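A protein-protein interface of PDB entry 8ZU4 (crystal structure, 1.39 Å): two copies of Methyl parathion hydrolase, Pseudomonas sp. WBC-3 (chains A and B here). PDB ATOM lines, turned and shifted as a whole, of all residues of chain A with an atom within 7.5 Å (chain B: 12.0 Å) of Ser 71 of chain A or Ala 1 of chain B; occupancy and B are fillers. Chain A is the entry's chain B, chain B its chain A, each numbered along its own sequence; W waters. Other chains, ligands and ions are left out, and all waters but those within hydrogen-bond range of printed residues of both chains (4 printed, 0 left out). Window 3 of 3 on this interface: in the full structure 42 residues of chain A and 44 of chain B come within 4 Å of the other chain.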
ATOM      1  N   PHE A  20      15.168 -17.200  22.658  1.00  0.00           N
ATOM      2  CA  PHE A  20      15.391 -18.276  21.700  1.00  0.00           C
ATOM      3  C   PHE A  20      15.424 -19.629  22.400  1.00  0.00           C
ATOM      4  O   PHE A  20      15.808 -19.743  23.570  1.00  0.00           O
ATOM      5  CB  PHE A  20      16.733 -18.103  20.976  1.00  0.00           C
ATOM      6  CG  PHE A  20      16.821 -16.896  20.071  1.00  0.00           C
ATOM      7  CD1 PHE A  20      15.756 -16.033  19.891  1.00  0.00           C
ATOM      8  CD2 PHE A  20      18.020 -16.612  19.425  1.00  0.00           C
ATOM      9  CE1 PHE A  20      15.868 -14.932  19.052  1.00  0.00           C
ATOM     10  CE2 PHE A  20      18.142 -15.504  18.591  1.00  0.00           C
ATOM     11  CZ  PHE A  20      17.068 -14.666  18.410  1.00  0.00           C
ATOM     12  N   ASN A  68      15.604 -22.102  17.436  1.00  0.00           N
ATOM     13  CA  ASN A  68      14.287 -21.566  17.126  1.00  0.00           C
ATOM     14  C   ASN A  68      14.232 -20.148  17.681  1.00  0.00           C
ATOM     15  O   ASN A  68      14.147 -19.951  18.900  1.00  0.00           O
ATOM     16  CB  ASN A  68      13.172 -22.442  17.690  1.00  0.00           C
ATOM     17  CG  ASN A  68      11.807 -22.063  17.151  1.00  0.00           C
ATOM     18  OD1 ASN A  68      11.573 -20.910  16.776  1.00  0.00           O
ATOM     19  ND2 ASN A  68      10.897 -23.029  17.099  1.00  0.00           N
ATOM     20  N   THR A  69      14.294 -19.163  16.782  1.00  0.00           N
ATOM     21  CA  THR A  69      14.263 -17.767  17.186  1.00  0.00           C
ATOM     22  C   THR A  69      12.857 -17.283  17.491  1.00  0.00           C
ATOM     23  O   THR A  69      12.693 -16.150  17.961  1.00  0.00           O
ATOM     24  CB  THR A  69      14.853 -16.878  16.092  1.00  0.00           C
ATOM     25  OG1 THR A  69      13.933 -16.808  14.994  1.00  0.00           O
ATOM     26  CG2 THR A  69      16.185 -17.425  15.618  1.00  0.00           C
ATOM     27  N   GLY A  70      11.844 -18.112  17.232  1.00  0.00           N
ATOM     28  CA  GLY A  70      10.455 -17.736  17.322  1.00  0.00           C
ATOM     29  C   GLY A  70       9.848 -17.354  15.986  1.00  0.00           C
ATOM     30  O   GLY A  70       8.641 -17.519  15.791  1.00  0.00           O
ATOM     31  N   SER A  71      10.668 -16.863  15.055  1.00  0.00           N
ATOM     32  CA  SER A  71      10.220 -16.596  13.696  1.00  0.00           C
ATOM     33  C   SER A  71      10.920 -17.441  12.644  1.00  0.00           C
ATOM     34  O   SER A  71      10.417 -17.530  11.516  1.00  0.00           O
ATOM     35  CB  SER A  71      10.375 -15.106  13.346  1.00  0.00           C
ATOM     36  OG  SER A  71      11.738 -14.719  13.342  1.00  0.00           O
ATOM     37  N   LYS A  72      12.054 -18.060  12.972  1.00  0.00           N
ATOM     38  CA  LYS A  72      12.761 -18.945  12.058  1.00  0.00           C
ATOM     39  C   LYS A  72      13.303 -20.133  12.835  1.00  0.00           C
ATOM     40  O   LYS A  72      13.604 -20.032  14.027  1.00  0.00           O
ATOM     41  CB  LYS A  72      13.911 -18.218  11.340  1.00  0.00           C
ATOM     42  CG  LYS A  72      13.436 -17.196  10.311  1.00  0.00           C
ATOM     43  CD  LYS A  72      13.233 -17.842   8.943  1.00  0.00           C
ATOM     44  CE  LYS A  72      12.246 -17.060   8.079  1.00  0.00           C
ATOM     45  NZ  LYS A  72      12.501 -15.601   8.159  1.00  0.00           N
ATOM     46  N   LEU A  73      13.408 -21.266  12.148  1.00  0.00           N
ATOM     47  CA  LEU A  73      14.018 -22.470  12.697  1.00  0.00           C
ATOM     48  C   LEU A  73      15.270 -22.757  11.883  1.00  0.00           C
ATOM     49  O   LEU A  73      15.181 -23.041  10.683  1.00  0.00           O
ATOM     50  CB  LEU A  73      13.046 -23.647  12.627  1.00  0.00           C
ATOM     51  CG  LEU A  73      13.520 -24.921  13.322  1.00  0.00           C
ATOM     52  CD1 LEU A  73      13.674 -24.696  14.828  1.00  0.00           C
ATOM     53  CD2 LEU A  73      12.566 -26.076  13.027  1.00  0.00           C
ATOM     54  N   VAL A  74      16.429 -22.686  12.536  1.00  0.00           N
ATOM     55  CA  VAL A  74      17.726 -22.768  11.879  1.00  0.00           C
ATOM     56  C   VAL A  74      18.480 -23.944  12.467  1.00  0.00           C
ATOM     57  O   VAL A  74      18.487 -24.137  13.685  1.00  0.00           O
ATOM     58  CB  VAL A  74      18.521 -21.464  12.099  1.00  0.00           C
ATOM     59  CG1 VAL A  74      19.892 -21.571  11.458  1.00  0.00           C
ATOM     60  CG2 VAL A  74      17.746 -20.278  11.547  1.00  0.00           C
ATOM     61  N   GLN A 104      10.193 -28.398   8.696  1.00  0.00           N
ATOM     62  CA  GLN A 104      10.054 -27.112   9.372  1.00  0.00           C
ATOM     63  C   GLN A 104      11.341 -26.299   9.394  1.00  0.00           C
ATOM     64  O   GLN A 104      11.289 -25.115   9.745  1.00  0.00           O
ATOM     65  CB  GLN A 104       9.613 -27.310  10.818  1.00  0.00           C
ATOM     66  CG  GLN A 104       8.268 -27.978  10.989  1.00  0.00           C
ATOM     67  CD  GLN A 104       7.931 -28.140  12.458  1.00  0.00           C
ATOM     68  OE1 GLN A 104       8.436 -29.050  13.123  1.00  0.00           O
ATOM     69  NE2 GLN A 104       7.073 -27.265  12.971  1.00  0.00           N
ATOM     70  N   ASP A 106      14.001 -23.885   8.317  1.00  0.00           N
ATOM     71  CA  ASP A 106      14.003 -22.807   7.335  1.00  0.00           C
ATOM     72  C   ASP A 106      15.371 -22.593   6.713  1.00  0.00           C
ATOM     73  O   ASP A 106      15.472 -22.351   5.502  1.00  0.00           O
ATOM     74  CB  ASP A 106      13.538 -21.507   7.982  1.00  0.00           C
ATOM     75  CG  ASP A 106      12.129 -21.606   8.541  1.00  0.00           C
ATOM     76  OD1 ASP A 106      11.226 -22.062   7.800  1.00  0.00           O
ATOM     77  OD2 ASP A 106      11.918 -21.203   9.707  1.00  0.00           O
ATOM     78  N   VAL A 188      19.833 -14.558   9.523  1.00  0.00           N
ATOM     79  CA  VAL A 188      18.513 -14.279  10.102  1.00  0.00           C
ATOM     80  C   VAL A 188      18.648 -13.509  11.415  1.00  0.00           C
ATOM     81  O   VAL A 188      19.649 -13.677  12.132  1.00  0.00           O
ATOM     82  CB  VAL A 188      17.674 -15.558  10.278  1.00  0.00           C
ATOM     83  CG1 VAL A 188      17.561 -16.308   8.964  1.00  0.00           C
ATOM     84  CG2 VAL A 188      18.250 -16.445  11.382  1.00  0.00           C
ATOM     85  N   PRO A 189      17.689 -12.635  11.753  1.00  0.00           N
ATOM     86  CA  PRO A 189      17.795 -11.862  13.001  1.00  0.00           C
ATOM     87  C   PRO A 189      18.131 -12.709  14.218  1.00  0.00           C
ATOM     88  O   PRO A 189      17.435 -13.682  14.531  1.00  0.00           O
ATOM     89  CB  PRO A 189      16.410 -11.212  13.126  1.00  0.00           C
ATOM     90  CG  PRO A 189      15.967 -11.061  11.693  1.00  0.00           C
ATOM     91  CD  PRO A 189      16.482 -12.279  10.983  1.00  0.00           C
ATOM     92  N   ALA B   1       5.775 -19.556  11.186  1.00  0.00           N
ATOM     93  CA  ALA B   1       6.923 -19.864  12.037  1.00  0.00           C
ATOM     94  C   ALA B   1       6.705 -21.124  12.879  1.00  0.00           C
ATOM     95  O   ALA B   1       5.638 -21.310  13.469  1.00  0.00           O
ATOM     96  CB  ALA B   1       7.246 -18.680  12.938  1.00  0.00           C
ATOM     97  N   ALA B   2       7.722 -21.979  12.948  1.00  0.00           N
ATOM     98  CA  ALA B   2       7.615 -23.193  13.752  1.00  0.00           C
ATOM     99  C   ALA B   2       7.514 -22.824  15.228  1.00  0.00           C
ATOM    100  O   ALA B   2       8.361 -22.080  15.735  1.00  0.00           O
ATOM    101  CB  ALA B   2       8.846 -24.071  13.538  1.00  0.00           C
ATOM    102  N   PRO B   3       6.502 -23.307  15.945  1.00  0.00           N
ATOM    103  CA  PRO B   3       6.411 -23.002  17.378  1.00  0.00           C
ATOM    104  C   PRO B   3       7.576 -23.597  18.145  1.00  0.00           C
ATOM    105  O   PRO B   3       8.107 -24.654  17.798  1.00  0.00           O
ATOM    106  CB  PRO B   3       5.097 -23.662  17.814  1.00  0.00           C
ATOM    107  CG  PRO B   3       4.466 -24.227  16.594  1.00  0.00           C
ATOM    108  CD  PRO B   3       5.261 -23.871  15.393  1.00  0.00           C
ATOM    109  N   GLN B   4       7.976 -22.912  19.209  1.00  0.00           N
ATOM    110  CA  GLN B   4       8.954 -23.511  20.099  1.00  0.00           C
ATOM    111  C   GLN B   4       8.302 -24.648  20.872  1.00  0.00           C
ATOM    112  O   GLN B   4       7.083 -24.678  21.062  1.00  0.00           O
ATOM    113  CB  GLN B   4       9.530 -22.463  21.047  1.00  0.00           C
ATOM    114  CG  GLN B   4      10.249 -21.337  20.309  1.00  0.00           C
ATOM    115  CD  GLN B   4      10.914 -20.368  21.256  1.00  0.00           C
ATOM    116  OE1 GLN B   4      10.620 -20.348  22.450  1.00  0.00           O
ATOM    117  NE2 GLN B   4      11.809 -19.549  20.730  1.00  0.00           N
ATOM    118  N   VAL B   5       9.119 -25.606  21.291  1.00  0.00           N
ATOM    119  CA  VAL B   5       8.644 -26.775  22.023  1.00  0.00           C
ATOM    120  C   VAL B   5       8.843 -26.610  23.522  1.00  0.00           C
ATOM    121  O   VAL B   5       7.906 -26.783  24.302  1.00  0.00           O
ATOM    122  CB  VAL B   5       9.307 -28.066  21.487  1.00  0.00           C
ATOM    123  CG1 VAL B   5       8.811 -29.281  22.250  1.00  0.00           C
ATOM    124  CG2 VAL B   5       9.017 -28.232  20.005  1.00  0.00           C
ATOM    125  N   ARG B   6      10.064 -26.256  23.934  1.00  0.00           N
ATOM    126  CA  ARG B   6      10.364 -25.885  25.320  1.00  0.00           C
ATOM    127  C   ARG B   6      10.052 -27.000  26.317  1.00  0.00           C
ATOM    128  O   ARG B   6       9.472 -26.771  27.379  1.00  0.00           O
ATOM    129  CB  ARG B   6       9.682 -24.576  25.716  1.00  0.00           C
ATOM    130  CG  ARG B   6      10.183 -23.388  24.962  1.00  0.00           C
ATOM    131  CD  ARG B   6      10.005 -22.128  25.785  1.00  0.00           C
ATOM    132  NE  ARG B   6      10.410 -20.952  25.028  1.00  0.00           N
ATOM    133  CZ  ARG B   6      10.745 -19.790  25.571  1.00  0.00           C
ATOM    134  NH1 ARG B   6      10.701 -19.602  26.882  1.00  0.00           N
ATOM    135  NH2 ARG B   6      11.140 -18.796  24.779  1.00  0.00           N
HETATM  136  O   HOH W   1      10.081 -21.140  11.429  1.00  0.00           O
HETATM  137  O   HOH W   2      10.285 -20.554  14.248  1.00  0.00           O
HETATM  138  O   HOH W   3       7.578 -19.561  16.836  1.00  0.00           O
HETATM  139  O   HOH W   4       7.325 -26.738  16.059  1.00  0.00           O
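The backbone carbonyl oxygen (O) of Ala 2 of chain B lies within hydrogen-bond range of the side-chain amide nitrogen (ND2) of Asn 68 of chain A, 3.0 Å away. O of Pro 3 of chain B lies within hydrogen-bond range of ND2 of Asn 68 of chain A (3.3 Å). The backbone carbonyl oxygen of Asn 68 of chain A sits at hydrogen-bond distance from the side-chain amide nitrogen of Gln 4 of chain B (3.0 Å).
OE1 of Gln 4 of chain B is in hydrogen-bond range of NE of Arg 6 of chain B (2.7 Å). The side-chain amide oxygen of Asn 68 of chain A sits at hydrogen-bond distance from the backbone NH of Gly 70 of chain A (2.8 Å). OG1 of Thr 69 of chain A lies within hydrogen-bond range of N of Ser 71 of chain A (3.3 Å).
Phe 20 of chain A touches Gln 4 of chain B. O of Gly 70 of chain A touches CB of Ala 1 of chain B, at 3.4 Å. Gly 70 of chain A touches Gln 4 of chain B. O of Ser 71 of chain A touches CB of Ala 1 of chain B, 3.7 Å away. NE2 of Gln 104 of chain A touches CB of Ala 2 of chain B, 3.7 Å away.
Of chain B, only Ala 1 comes within 4 Å of Ser 71 of chain A. Of the printed residues of chain B, Asn 68 of chain A touches Ala 2 (3.0 Å), Pro 3 (3.3 Å) and Gln 4 (3.0 Å). No residue of chain B comes within 4 Å of Thr 69 of chain A. No residue of chain B comes within 4 Å of Lys 72 of chain A. Of the printed residues of chain B, Phe 20 of chain A touches Gln 4 (3.9 Å). Of the printed residues of chain A, Pro 3 of chain B touches Asn 68 (3.3 Å). Of the printed residues of chain B, Gln 104 of chain A touches Ala 2. Asp 106 of chain A touches none of the printed residues of chain B. Leu 73 of chain A touches none of the printed residues of chain B. The nearest residue of chain B that does not touch Ser 71 of chain A is Ala 2 of chain B (5.4 Å). The nearest residue of chain A that does not touch Ala 1 of chain B is Lys 72 of chain A (4.8 Å).
Printed residues of chain A that touch a printed residue of chain B: Phe 20, Asn 68, Gly 70, Ser 71 and Gln 104. Among the printed residues, 8 pairs touch across the chains.
No position is printed for both chains.
Water W1 lies within hydrogen-bond range of OD2 of Asp 106 of chain A (2.5 Å), N of Ala 2 of chain B (2.9 Å) and N of Leu 73 of chain A (3.4 Å). Water W3 bridges the backbone carbonyl oxygen (O) of Gly 70 of chain A (2.5 Å) and the backbone carbonyl oxygen (O) of Ala 2 of chain B (2.9 Å). Water W4 lies within hydrogen-bond range of O of Pro 3 of chain B (2.8 Å) and NE2 of Gln 104 of chain A (3.1 Å). Water W2 lies within hydrogen-bond range of OD1 of Asn 68 of chain A (2.9 Å), O of Ala 2 of chain B (2.9 Å) and N of Lys 72 of chain A (3.3 Å).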
